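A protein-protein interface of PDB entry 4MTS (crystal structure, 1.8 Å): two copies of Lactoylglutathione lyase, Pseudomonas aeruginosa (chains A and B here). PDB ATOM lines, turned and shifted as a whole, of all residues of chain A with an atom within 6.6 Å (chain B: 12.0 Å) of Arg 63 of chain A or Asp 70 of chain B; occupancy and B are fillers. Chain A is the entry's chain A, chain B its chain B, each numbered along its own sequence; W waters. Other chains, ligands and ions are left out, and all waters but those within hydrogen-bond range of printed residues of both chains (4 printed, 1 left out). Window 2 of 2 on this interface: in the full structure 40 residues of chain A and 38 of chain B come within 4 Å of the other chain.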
ATOM      1  N   ARG A   9      -9.748  15.118  -9.848  1.00  0.00           N
ATOM      2  CA  ARG A   9     -10.889  14.888 -10.764  1.00  0.00           C
ATOM      3  C   ARG A   9     -10.704  15.751 -12.033  1.00  0.00           C
ATOM      4  O   ARG A   9     -10.327  16.917 -11.949  1.00  0.00           O
ATOM      5  CB  ARG A   9     -12.212  15.221 -10.075  1.00  0.00           C
ATOM      6  CG  ARG A   9     -12.486  14.329  -8.849  1.00  0.00           C
ATOM      7  CD  ARG A   9     -13.840  14.620  -8.205  1.00  0.00           C
ATOM      8  NE  ARG A   9     -13.989  13.796  -6.997  1.00  0.00           N
ATOM      9  CZ  ARG A   9     -13.592  14.170  -5.789  1.00  0.00           C
ATOM     10  NH1 ARG A   9     -13.056  15.369  -5.604  1.00  0.00           N
ATOM     11  NH2 ARG A   9     -13.696  13.332  -4.757  1.00  0.00           N
ATOM     12  N   VAL A  10     -10.930  15.152 -13.217  1.00  0.00           N
ATOM     13  CA  VAL A  10     -10.720  15.783 -14.524  1.00  0.00           C
ATOM     14  C   VAL A  10     -11.994  15.721 -15.353  1.00  0.00           C
ATOM     15  O   VAL A  10     -12.756  14.754 -15.225  1.00  0.00           O
ATOM     16  CB  VAL A  10      -9.493  15.175 -15.280  1.00  0.00           C
ATOM     17  CG1 VAL A  10      -8.209  15.368 -14.463  1.00  0.00           C
ATOM     18  CG2 VAL A  10      -9.708  13.696 -15.604  1.00  0.00           C
ATOM     19  N   ALA A  11     -12.194  16.734 -16.207  1.00  0.00           N
ATOM     20  CA  ALA A  11     -13.394  16.828 -17.041  1.00  0.00           C
ATOM     21  C   ALA A  11     -13.316  15.869 -18.225  1.00  0.00           C
ATOM     22  O   ALA A  11     -14.335  15.334 -18.650  1.00  0.00           O
ATOM     23  CB  ALA A  11     -13.598  18.265 -17.520  1.00  0.00           C
ATOM     24  N   HIS A  59     -12.472  10.338 -13.512  1.00  0.00           N
ATOM     25  CA  HIS A  59     -13.422  10.979 -14.402  1.00  0.00           C
ATOM     26  C   HIS A  59     -14.767  10.313 -14.195  1.00  0.00           C
ATOM     27  O   HIS A  59     -14.878   9.110 -14.388  1.00  0.00           O
ATOM     28  CB  HIS A  59     -12.950  10.859 -15.879  1.00  0.00           C
ATOM     29  CG  HIS A  59     -13.973  11.327 -16.853  1.00  0.00           C
ATOM     30  ND1 HIS A  59     -14.496  10.468 -17.807  1.00  0.00           N
ATOM     31  CD2 HIS A  59     -14.608  12.521 -16.942  1.00  0.00           C
ATOM     32  CE1 HIS A  59     -15.388  11.177 -18.482  1.00  0.00           C
ATOM     33  NE2 HIS A  59     -15.513  12.402 -17.991  1.00  0.00           N
ATOM     34  N   ASN A  60     -15.770  11.088 -13.757  1.00  0.00           N
ATOM     35  CA  ASN A  60     -17.145  10.629 -13.559  1.00  0.00           C
ATOM     36  C   ASN A  60     -17.788  10.861 -14.921  1.00  0.00           C
ATOM     37  O   ASN A  60     -17.731  11.986 -15.443  1.00  0.00           O
ATOM     38  CB  ASN A  60     -17.810  11.474 -12.446  1.00  0.00           C
ATOM     39  CG  ASN A  60     -17.187  11.228 -11.088  1.00  0.00           C
ATOM     40  OD1 ASN A  60     -17.303  10.129 -10.521  1.00  0.00           O
ATOM     41  ND2 ASN A  60     -16.481  12.236 -10.545  1.00  0.00           N
ATOM     42  N   TRP A  61     -18.298   9.787 -15.559  1.00  0.00           N
ATOM     43  CA  TRP A  61     -18.828   9.839 -16.914  1.00  0.00           C
ATOM     44  C   TRP A  61     -19.940  10.845 -17.103  1.00  0.00           C
ATOM     45  O   TRP A  61     -20.105  11.362 -18.214  1.00  0.00           O
ATOM     46  CB  TRP A  61     -19.330   8.450 -17.361  1.00  0.00           C
ATOM     47  CG  TRP A  61     -18.289   7.377 -17.297  1.00  0.00           C
ATOM     48  CD1 TRP A  61     -16.955   7.528 -17.034  1.00  0.00           C
ATOM     49  CD2 TRP A  61     -18.480   6.000 -17.606  1.00  0.00           C
ATOM     50  NE1 TRP A  61     -16.313   6.316 -17.133  1.00  0.00           N
ATOM     51  CE2 TRP A  61     -17.225   5.359 -17.468  1.00  0.00           C
ATOM     52  CE3 TRP A  61     -19.587   5.241 -18.002  1.00  0.00           C
ATOM     53  CZ2 TRP A  61     -17.055   3.988 -17.680  1.00  0.00           C
ATOM     54  CZ3 TRP A  61     -19.425   3.874 -18.175  1.00  0.00           C
ATOM     55  CH2 TRP A  61     -18.165   3.269 -18.045  1.00  0.00           C
ATOM     56  N   ASP A  62     -20.732  11.071 -16.062  1.00  0.00           N
ATOM     57  CA  ASP A  62     -21.863  11.991 -16.155  1.00  0.00           C
ATOM     58  C   ASP A  62     -21.601  13.420 -15.661  1.00  0.00           C
ATOM     59  O   ASP A  62     -22.531  14.225 -15.639  1.00  0.00           O
ATOM     60  CB  ASP A  62     -23.134  11.359 -15.562  1.00  0.00           C
ATOM     61  CG  ASP A  62     -23.380   9.956 -16.107  1.00  0.00           C
ATOM     62  OD1 ASP A  62     -23.366   8.999 -15.306  1.00  0.00           O
ATOM     63  OD2 ASP A  62     -23.466   9.810 -17.334  1.00  0.00           O
ATOM     64  N   ARG A  63     -20.343  13.736 -15.276  1.00  0.00           N
ATOM     65  CA  ARG A  63     -19.908  15.092 -14.854  1.00  0.00           C
ATOM     66  C   ARG A  63     -19.177  15.713 -16.032  1.00  0.00           C
ATOM     67  O   ARG A  63     -18.486  14.997 -16.757  1.00  0.00           O
ATOM     68  CB  ARG A  63     -18.939  15.039 -13.648  1.00  0.00           C
ATOM     69  CG  ARG A  63     -19.579  14.730 -12.291  1.00  0.00           C
ATOM     70  CD  ARG A  63     -20.421  15.856 -11.715  1.00  0.00           C
ATOM     71  NE  ARG A  63     -19.658  17.070 -11.398  1.00  0.00           N
ATOM     72  CZ  ARG A  63     -19.164  17.353 -10.198  1.00  0.00           C
ATOM     73  NH1 ARG A  63     -19.292  16.490  -9.198  1.00  0.00           N
ATOM     74  NH2 ARG A  63     -18.526  18.492  -9.992  1.00  0.00           N
ATOM     75  N   ASP A  64     -19.308  17.026 -16.226  1.00  0.00           N
ATOM     76  CA  ASP A  64     -18.686  17.722 -17.355  1.00  0.00           C
ATOM     77  C   ASP A  64     -17.542  18.636 -16.944  1.00  0.00           C
ATOM     78  O   ASP A  64     -16.918  19.290 -17.790  1.00  0.00           O
ATOM     79  CB  ASP A  64     -19.748  18.543 -18.120  1.00  0.00           C
ATOM     80  CG  ASP A  64     -20.802  17.741 -18.852  1.00  0.00           C
ATOM     81  OD1 ASP A  64     -20.435  16.744 -19.525  1.00  0.00           O
ATOM     82  OD2 ASP A  64     -21.989  18.141 -18.804  1.00  0.00           O
ATOM     83  N   GLY A  65     -17.303  18.705 -15.649  1.00  0.00           N
ATOM     84  CA  GLY A  65     -16.274  19.556 -15.088  1.00  0.00           C
ATOM     85  C   GLY A  65     -16.427  19.705 -13.592  1.00  0.00           C
ATOM     86  O   GLY A  65     -17.386  19.222 -12.981  1.00  0.00           O
ATOM     87  N   TYR A  66     -15.448  20.368 -13.009  1.00  0.00           N
ATOM     88  CA  TYR A  66     -15.340  20.582 -11.581  1.00  0.00           C
ATOM     89  C   TYR A  66     -15.043  22.052 -11.299  1.00  0.00           C
ATOM     90  O   TYR A  66     -14.764  22.829 -12.236  1.00  0.00           O
ATOM     91  CB  TYR A  66     -14.235  19.652 -11.042  1.00  0.00           C
ATOM     92  CG  TYR A  66     -14.586  18.199 -11.246  1.00  0.00           C
ATOM     93  CD1 TYR A  66     -14.231  17.533 -12.418  1.00  0.00           C
ATOM     94  CD2 TYR A  66     -15.397  17.524 -10.337  1.00  0.00           C
ATOM     95  CE1 TYR A  66     -14.634  16.220 -12.654  1.00  0.00           C
ATOM     96  CE2 TYR A  66     -15.832  16.229 -10.580  1.00  0.00           C
ATOM     97  CZ  TYR A  66     -15.409  15.562 -11.714  1.00  0.00           C
ATOM     98  OH  TYR A  66     -15.798  14.267 -11.912  1.00  0.00           O
ATOM     99  N   THR A  67     -15.199  22.463 -10.027  1.00  0.00           N
ATOM    100  CA  THR A  67     -14.891  23.818  -9.620  1.00  0.00           C
ATOM    101  C   THR A  67     -13.597  23.730  -8.838  1.00  0.00           C
ATOM    102  O   THR A  67     -13.494  22.885  -7.956  1.00  0.00           O
ATOM    103  CB  THR A  67     -16.044  24.425  -8.801  1.00  0.00           C
ATOM    104  OG1 THR A  67     -17.222  24.464  -9.610  1.00  0.00           O
ATOM    105  CG2 THR A  67     -15.733  25.839  -8.317  1.00  0.00           C
ATOM    106  N   GLN A  68     -12.606  24.550  -9.202  1.00  0.00           N
ATOM    107  CA  GLN A  68     -11.328  24.612  -8.488  1.00  0.00           C
ATOM    108  C   GLN A  68     -11.400  25.673  -7.412  1.00  0.00           C
ATOM    109  O   GLN A  68     -11.932  26.755  -7.631  1.00  0.00           O
ATOM    110  CB  GLN A  68     -10.175  24.971  -9.436  1.00  0.00           C
ATOM    111  CG  GLN A  68      -9.934  23.960 -10.562  1.00  0.00           C
ATOM    112  CD  GLN A  68      -9.970  22.535 -10.063  1.00  0.00           C
ATOM    113  OE1 GLN A  68      -9.543  22.227  -8.942  1.00  0.00           O
ATOM    114  NE2 GLN A  68     -10.544  21.645 -10.858  1.00  0.00           N
ATOM    115  N   GLY A  69     -10.873  25.348  -6.250  1.00  0.00           N
ATOM    116  CA  GLY A  69     -10.780  26.325  -5.176  1.00  0.00           C
ATOM    117  C   GLY A  69      -9.347  26.793  -5.037  1.00  0.00           C
ATOM    118  O   GLY A  69      -8.522  26.641  -5.957  1.00  0.00           O
ATOM    119  N   TYR A 119      -5.088  22.432 -13.291  1.00  0.00           N
ATOM    120  CA  TYR A 119      -4.290  22.083 -12.110  1.00  0.00           C
ATOM    121  C   TYR A 119      -2.860  22.476 -12.368  1.00  0.00           C
ATOM    122  O   TYR A 119      -2.343  22.295 -13.487  1.00  0.00           O
ATOM    123  CB  TYR A 119      -4.350  20.585 -11.829  1.00  0.00           C
ATOM    124  CG  TYR A 119      -5.721  20.109 -11.443  1.00  0.00           C
ATOM    125  CD1 TYR A 119      -6.283  20.463 -10.217  1.00  0.00           C
ATOM    126  CD2 TYR A 119      -6.452  19.274 -12.284  1.00  0.00           C
ATOM    127  CE1 TYR A 119      -7.540  20.005  -9.837  1.00  0.00           C
ATOM    128  CE2 TYR A 119      -7.708  18.793 -11.907  1.00  0.00           C
ATOM    129  CZ  TYR A 119      -8.232  19.139 -10.666  1.00  0.00           C
ATOM    130  OH  TYR A 119      -9.447  18.680 -10.248  1.00  0.00           O
ATOM    131  N   LEU B   8      -0.654  21.303  -0.374  1.00  0.00           N
ATOM    132  CA  LEU B   8      -1.961  21.744   0.135  1.00  0.00           C
ATOM    133  C   LEU B   8      -1.741  22.991   0.978  1.00  0.00           C
ATOM    134  O   LEU B   8      -0.778  23.054   1.768  1.00  0.00           O
ATOM    135  CB  LEU B   8      -2.606  20.673   1.042  1.00  0.00           C
ATOM    136  CG  LEU B   8      -2.805  19.293   0.363  1.00  0.00           C
ATOM    137  CD1 LEU B   8      -3.353  18.274   1.402  1.00  0.00           C
ATOM    138  CD2 LEU B   8      -3.780  19.420  -0.849  1.00  0.00           C
ATOM    139  N   TYR B  66      -9.322  28.824   3.458  1.00  0.00           N
ATOM    140  CA  TYR B  66      -9.335  28.629   2.005  1.00  0.00           C
ATOM    141  C   TYR B  66     -10.696  28.195   1.527  1.00  0.00           C
ATOM    142  O   TYR B  66     -11.458  27.587   2.287  1.00  0.00           O
ATOM    143  CB  TYR B  66      -8.274  27.578   1.608  1.00  0.00           C
ATOM    144  CG  TYR B  66      -6.886  28.093   1.896  1.00  0.00           C
ATOM    145  CD1 TYR B  66      -6.293  27.895   3.140  1.00  0.00           C
ATOM    146  CD2 TYR B  66      -6.240  28.939   0.995  1.00  0.00           C
ATOM    147  CE1 TYR B  66      -5.071  28.485   3.461  1.00  0.00           C
ATOM    148  CE2 TYR B  66      -5.004  29.500   1.292  1.00  0.00           C
ATOM    149  CZ  TYR B  66      -4.426  29.274   2.529  1.00  0.00           C
ATOM    150  OH  TYR B  66      -3.212  29.828   2.831  1.00  0.00           O
ATOM    151  N   THR B  67     -10.966  28.433   0.241  1.00  0.00           N
ATOM    152  CA  THR B  67     -12.211  28.022  -0.378  1.00  0.00           C
ATOM    153  C   THR B  67     -11.902  26.723  -1.097  1.00  0.00           C
ATOM    154  O   THR B  67     -11.095  26.710  -2.025  1.00  0.00           O
ATOM    155  CB  THR B  67     -12.721  29.089  -1.350  1.00  0.00           C
ATOM    156  OG1 THR B  67     -12.861  30.341  -0.667  1.00  0.00           O
ATOM    157  CG2 THR B  67     -14.041  28.701  -1.959  1.00  0.00           C
ATOM    158  N   GLN B  68     -12.505  25.634  -0.664  1.00  0.00           N
ATOM    159  CA  GLN B  68     -12.214  24.367  -1.312  1.00  0.00           C
ATOM    160  C   GLN B  68     -13.142  24.155  -2.486  1.00  0.00           C
ATOM    161  O   GLN B  68     -14.340  24.347  -2.349  1.00  0.00           O
ATOM    162  CB  GLN B  68     -12.342  23.188  -0.327  1.00  0.00           C
ATOM    163  CG  GLN B  68     -11.385  23.290   0.851  1.00  0.00           C
ATOM    164  CD  GLN B  68      -9.947  23.328   0.432  1.00  0.00           C
ATOM    165  OE1 GLN B  68      -9.573  22.796  -0.621  1.00  0.00           O
ATOM    166  NE2 GLN B  68      -9.106  23.962   1.252  1.00  0.00           N
ATOM    167  N   GLY B  69     -12.578  23.724  -3.615  1.00  0.00           N
ATOM    168  CA  GLY B  69     -13.396  23.385  -4.773  1.00  0.00           C
ATOM    169  C   GLY B  69     -13.712  21.899  -4.715  1.00  0.00           C
ATOM    170  O   GLY B  69     -13.462  21.243  -3.696  1.00  0.00           O
ATOM    171  N   ASP B  70     -14.240  21.335  -5.796  1.00  0.00           N
ATOM    172  CA  ASP B  70     -14.599  19.944  -5.777  1.00  0.00           C
ATOM    173  C   ASP B  70     -13.703  19.112  -6.694  1.00  0.00           C
ATOM    174  O   ASP B  70     -13.986  17.926  -6.904  1.00  0.00           O
ATOM    175  CB  ASP B  70     -16.107  19.798  -6.103  1.00  0.00           C
ATOM    176  CG  ASP B  70     -16.510  20.516  -7.383  1.00  0.00           C
ATOM    177  OD1 ASP B  70     -17.605  21.089  -7.417  1.00  0.00           O
ATOM    178  OD2 ASP B  70     -15.713  20.538  -8.318  1.00  0.00           O
ATOM    179  N   GLY B  71     -12.627  19.731  -7.215  1.00  0.00           N
ATOM    180  CA  GLY B  71     -11.678  19.058  -8.089  1.00  0.00           C
ATOM    181  C   GLY B  71     -10.674  18.173  -7.369  1.00  0.00           C
ATOM    182  O   GLY B  71     -10.470  17.014  -7.744  1.00  0.00           O
ATOM    183  N   TYR B  72     -10.054  18.697  -6.307  1.00  0.00           N
ATOM    184  CA  TYR B  72      -9.059  17.942  -5.525  1.00  0.00           C
ATOM    185  C   TYR B  72      -9.715  16.742  -4.843  1.00  0.00           C
ATOM    186  O   TYR B  72     -10.760  16.876  -4.220  1.00  0.00           O
ATOM    187  CB  TYR B  72      -8.380  18.844  -4.481  1.00  0.00           C
ATOM    188  CG  TYR B  72      -7.426  18.046  -3.627  1.00  0.00           C
ATOM    189  CD1 TYR B  72      -6.328  17.402  -4.196  1.00  0.00           C
ATOM    190  CD2 TYR B  72      -7.702  17.801  -2.283  1.00  0.00           C
ATOM    191  CE1 TYR B  72      -5.483  16.611  -3.437  1.00  0.00           C
ATOM    192  CE2 TYR B  72      -6.856  17.004  -1.511  1.00  0.00           C
ATOM    193  CZ  TYR B  72      -5.722  16.460  -2.082  1.00  0.00           C
ATOM    194  OH  TYR B  72      -4.895  15.640  -1.354  1.00  0.00           O
ATOM    195  N   GLY B  73      -9.083  15.584  -4.959  1.00  0.00           N
ATOM    196  CA  GLY B  73      -9.648  14.350  -4.415  1.00  0.00           C
ATOM    197  C   GLY B  73      -9.186  14.029  -3.018  1.00  0.00           C
ATOM    198  O   GLY B  73      -9.883  14.338  -2.048  1.00  0.00           O
ATOM    199  N   HIS B  74      -7.989  13.417  -2.917  1.00  0.00           N
ATOM    200  CA  HIS B  74      -7.423  12.991  -1.627  1.00  0.00           C
ATOM    201  C   HIS B  74      -5.969  12.620  -1.804  1.00  0.00           C
ATOM    202  O   HIS B  74      -5.447  12.626  -2.920  1.00  0.00           O
ATOM    203  CB  HIS B  74      -8.208  11.752  -1.105  1.00  0.00           C
ATOM    204  CG  HIS B  74      -8.237  10.592  -2.064  1.00  0.00           C
ATOM    205  ND1 HIS B  74      -9.369  10.334  -2.851  1.00  0.00           N
ATOM    206  CD2 HIS B  74      -7.300   9.649  -2.335  1.00  0.00           C
ATOM    207  CE1 HIS B  74      -9.069   9.258  -3.569  1.00  0.00           C
ATOM    208  NE2 HIS B  74      -7.832   8.838  -3.330  1.00  0.00           N
ATOM    209  N   ASP B 117      -8.038  20.998   7.939  1.00  0.00           N
ATOM    210  CA  ASP B 117      -8.529  21.871   6.868  1.00  0.00           C
ATOM    211  C   ASP B 117      -9.629  21.182   6.056  1.00  0.00           C
ATOM    212  O   ASP B 117     -10.156  21.793   5.136  1.00  0.00           O
ATOM    213  CB  ASP B 117      -7.386  22.284   5.941  1.00  0.00           C
ATOM    214  CG  ASP B 117      -6.484  23.278   6.621  1.00  0.00           C
ATOM    215  OD1 ASP B 117      -6.808  24.475   6.585  1.00  0.00           O
ATOM    216  OD2 ASP B 117      -5.556  22.838   7.327  1.00  0.00           O
ATOM    217  N   GLY B 118      -9.969  19.940   6.403  1.00  0.00           N
ATOM    218  CA  GLY B 118     -11.041  19.246   5.708  1.00  0.00           C
ATOM    219  C   GLY B 118     -10.587  18.385   4.552  1.00  0.00           C
ATOM    220  O   GLY B 118     -11.424  17.752   3.898  1.00  0.00           O
ATOM    221  N   TYR B 119      -9.265  18.327   4.292  1.00  0.00           N
ATOM    222  CA  TYR B 119      -8.690  17.492   3.202  1.00  0.00           C
ATOM    223  C   TYR B 119      -8.786  16.018   3.606  1.00  0.00           C
ATOM    224  O   TYR B 119      -8.586  15.678   4.766  1.00  0.00           O
ATOM    225  CB  TYR B 119      -7.210  17.846   2.938  1.00  0.00           C
ATOM    226  CG  TYR B 119      -6.984  19.271   2.507  1.00  0.00           C
ATOM    227  CD1 TYR B 119      -7.502  19.749   1.302  1.00  0.00           C
ATOM    228  CD2 TYR B 119      -6.161  20.119   3.243  1.00  0.00           C
ATOM    229  CE1 TYR B 119      -7.230  21.043   0.857  1.00  0.00           C
ATOM    230  CE2 TYR B 119      -5.892  21.417   2.810  1.00  0.00           C
ATOM    231  CZ  TYR B 119      -6.425  21.875   1.620  1.00  0.00           C
ATOM    232  OH  TYR B 119      -6.233  23.184   1.239  1.00  0.00           O
ATOM    233  N   LYS B 120      -9.085  15.140   2.643  1.00  0.00           N
ATOM    234  CA  LYS B 120      -9.268  13.722   2.946  1.00  0.00           C
ATOM    235  C   LYS B 120      -8.007  12.928   2.744  1.00  0.00           C
ATOM    236  O   LYS B 120      -7.287  13.126   1.753  1.00  0.00           O
ATOM    237  CB  LYS B 120     -10.404  13.120   2.103  1.00  0.00           C
ATOM    238  CG  LYS B 120     -11.781  13.616   2.544  1.00  0.00           C
ATOM    239  CD  LYS B 120     -12.829  13.115   1.561  1.00  0.00           C
ATOM    240  CE  LYS B 120     -14.168  12.864   2.206  1.00  0.00           C
ATOM    241  NZ  LYS B 120     -15.091  12.177   1.264  1.00  0.00           N
HETATM  242  O   HOH W   1     -12.571  14.399  -2.278  1.00  0.00           O
HETATM  243  O   HOH W   2     -16.288  16.427  -6.095  1.00  0.00           O
HETATM  244  O   HOH W   3     -11.907  11.414  -2.456  1.00  0.00           O
HETATM  245  O   HOH W   4      -9.166  23.660  -4.053  1.00  0.00           O
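Thr 67 of chain A touches Gly 69 of chain B, and with the chains exchanged Gly 69 of chain A touches Thr 67 of chain B.
Gly 69 of chain B touches its own counterpart, Gly 69 of chain A.
Positions printed for both chains: 66, 67, 68, 69 and 119.
Of the 15 pairs that touch across the chains among the printed residues, 3 have their exchanged pair printed and touching as well.
No residue of chain B comes within 4 Å of Asn 60 of chain A.
No residue of chain B comes within 4 Å of Asp 62 of chain A.
No residue of chain B comes within 4 Å of Asp 64 of chain A.
No residue of chain B comes within 4 Å of Gly 65 of chain A.
Of chain B, only Gly 69, Asp 70 and Gly 71 come within 4 Å of Thr 67 of chain A.
Of chain B, only Gly 71 comes within 4 Å of Gln 68 of chain A.
Printed residues of chain B within 4 Å of Tyr 119 of chain A: Gly 71 (3.1 Å) and Tyr 72 (3.99 Å).
Of the printed residues of chain A, Thr 67 of chain B touches Gly 69.
Of the printed residues of chain A, Gly 69 of chain B touches Thr 67 and Gly 69.
Of the printed residues of chain A, Asp 70 of chain B touches Arg 9 (3.0 Å), Arg 63 (3.8 Å), Tyr 66 (3.2 Å) and Thr 67 (2.6 Å).
Of the printed residues of chain A, Gly 71 of chain B touches Arg 9, Tyr 66, Thr 67, Gln 68 and Tyr 119.
Printed residues of chain A within 4 Å of Tyr 72 of chain B: Arg 9 and Tyr 119.
Asp 117 of chain B touches none of the printed residues of chain A.
Lys 120 of chain B touches none of the printed residues of chain A.
The nearest residue of chain A that does not touch Asp 70 of chain B is Gln 68 of chain A (5.0 Å).
Hydrophobic or aromatic side chains of chain A within 4 Å of the printed part of chain B: Tyr 66 and Tyr 119.
Among the printed residues, 15 pairs touch across the chains.
The backbone carbonyl oxygen (O) of Gly 65 of chain A is in hydrogen-bond range of the guanidinium group (NH2) of Arg 63 of chain A.
The side-chain amide nitrogen (ND2) of Asn 60 of chain A is in hydrogen-bond range of the side-chain hydroxyl (OH) of Tyr 66 of chain A, 2.5 Å away.
The side-chain hydroxyl (OH) of Tyr 72 of chain B sits close to the backbone carbonyl oxygen (O) of His 74 of chain B (3.4 Å).
The side-chain amide nitrogen of Gln 68 of chain A is in hydrogen-bond range of the side-chain hydroxyl of Tyr 119 of chain A, 3.2 Å away.
The backbone carbonyl oxygen (O) of Arg 9 of chain A sits at hydrogen-bond distance from the side-chain hydroxyl (OH) of Tyr 119 of chain A (2.6 Å).
N of Gly 71 of chain B lies within hydrogen-bond range of O of Thr 67 of chain A.
OD1 of Asp 70 of chain B is in salt-bridge range of NH2 of Arg 63 of chain A.
The backbone carbonyl oxygen of Gly 71 of chain B lies close to the side-chain hydroxyl of Tyr 119 of chain A (3.2 Å).
The guanidinium group (NH1) of Arg 9 of chain A is in hydrogen-bond range of the backbone carbonyl oxygen (O) of Asp 70 of chain B, at 3.0 Å.
The backbone NH (N) of Arg 9 of chain A is in hydrogen-bond range of the backbone carbonyl oxygen (O) of Gly 71 of chain B (2.9 Å).
The side-chain carboxylate of Asp 70 of chain B sits at hydrogen-bond distance from the backbone NH of Thr 67 of chain A (2.6 Å).
NH1 of Arg 9 of chain A lies within hydrogen-bond range of O of Tyr 72 of chain B, 3.1 Å away.
Water W1 bridges the backbone carbonyl oxygen of Gly 73 of chain B and the guanidinium group of Arg 9 of chain A.
Water W3 bridges a ring nitrogen (ND1) of His 74 of chain B (2.8 Å) and the guanidinium group (NH2) of Arg 9 of chain A (3.5 Å).
Water W2 bridges O of Asp 70 of chain B (2.9 Å) and NH1 of Arg 9 of chain A (3.4 Å).
Water W4 lies within hydrogen-bond range of the backbone NH of Gly 69 of chain A (3.3 Å) and the backbone NH of Gly 69 of chain B (3.4 Å).
Arg 9 of chain A touches Gly 73 of chain B.
Tyr 66 of chain A touches Asp 70 of chain B.
Tyr 66 of chain A touches Gly 71 of chain B (CB to CA, 3.95 Å).
Thr 67 of chain A touches Gly 69 of chain B (O to CA, 3.2 Å).
Gln 68 of chain A touches Gly 71 of chain B (OE1 to CA, 3.9 Å).
CA of Gly 69 of chain A touches O of Thr 67 of chain B, 3.2 Å away.
Gly 69 of chain A touches Gly 69 of chain B.
Tyr 72 of chain B touches Tyr 119 of chain A (N to OH, 3.99 Å).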
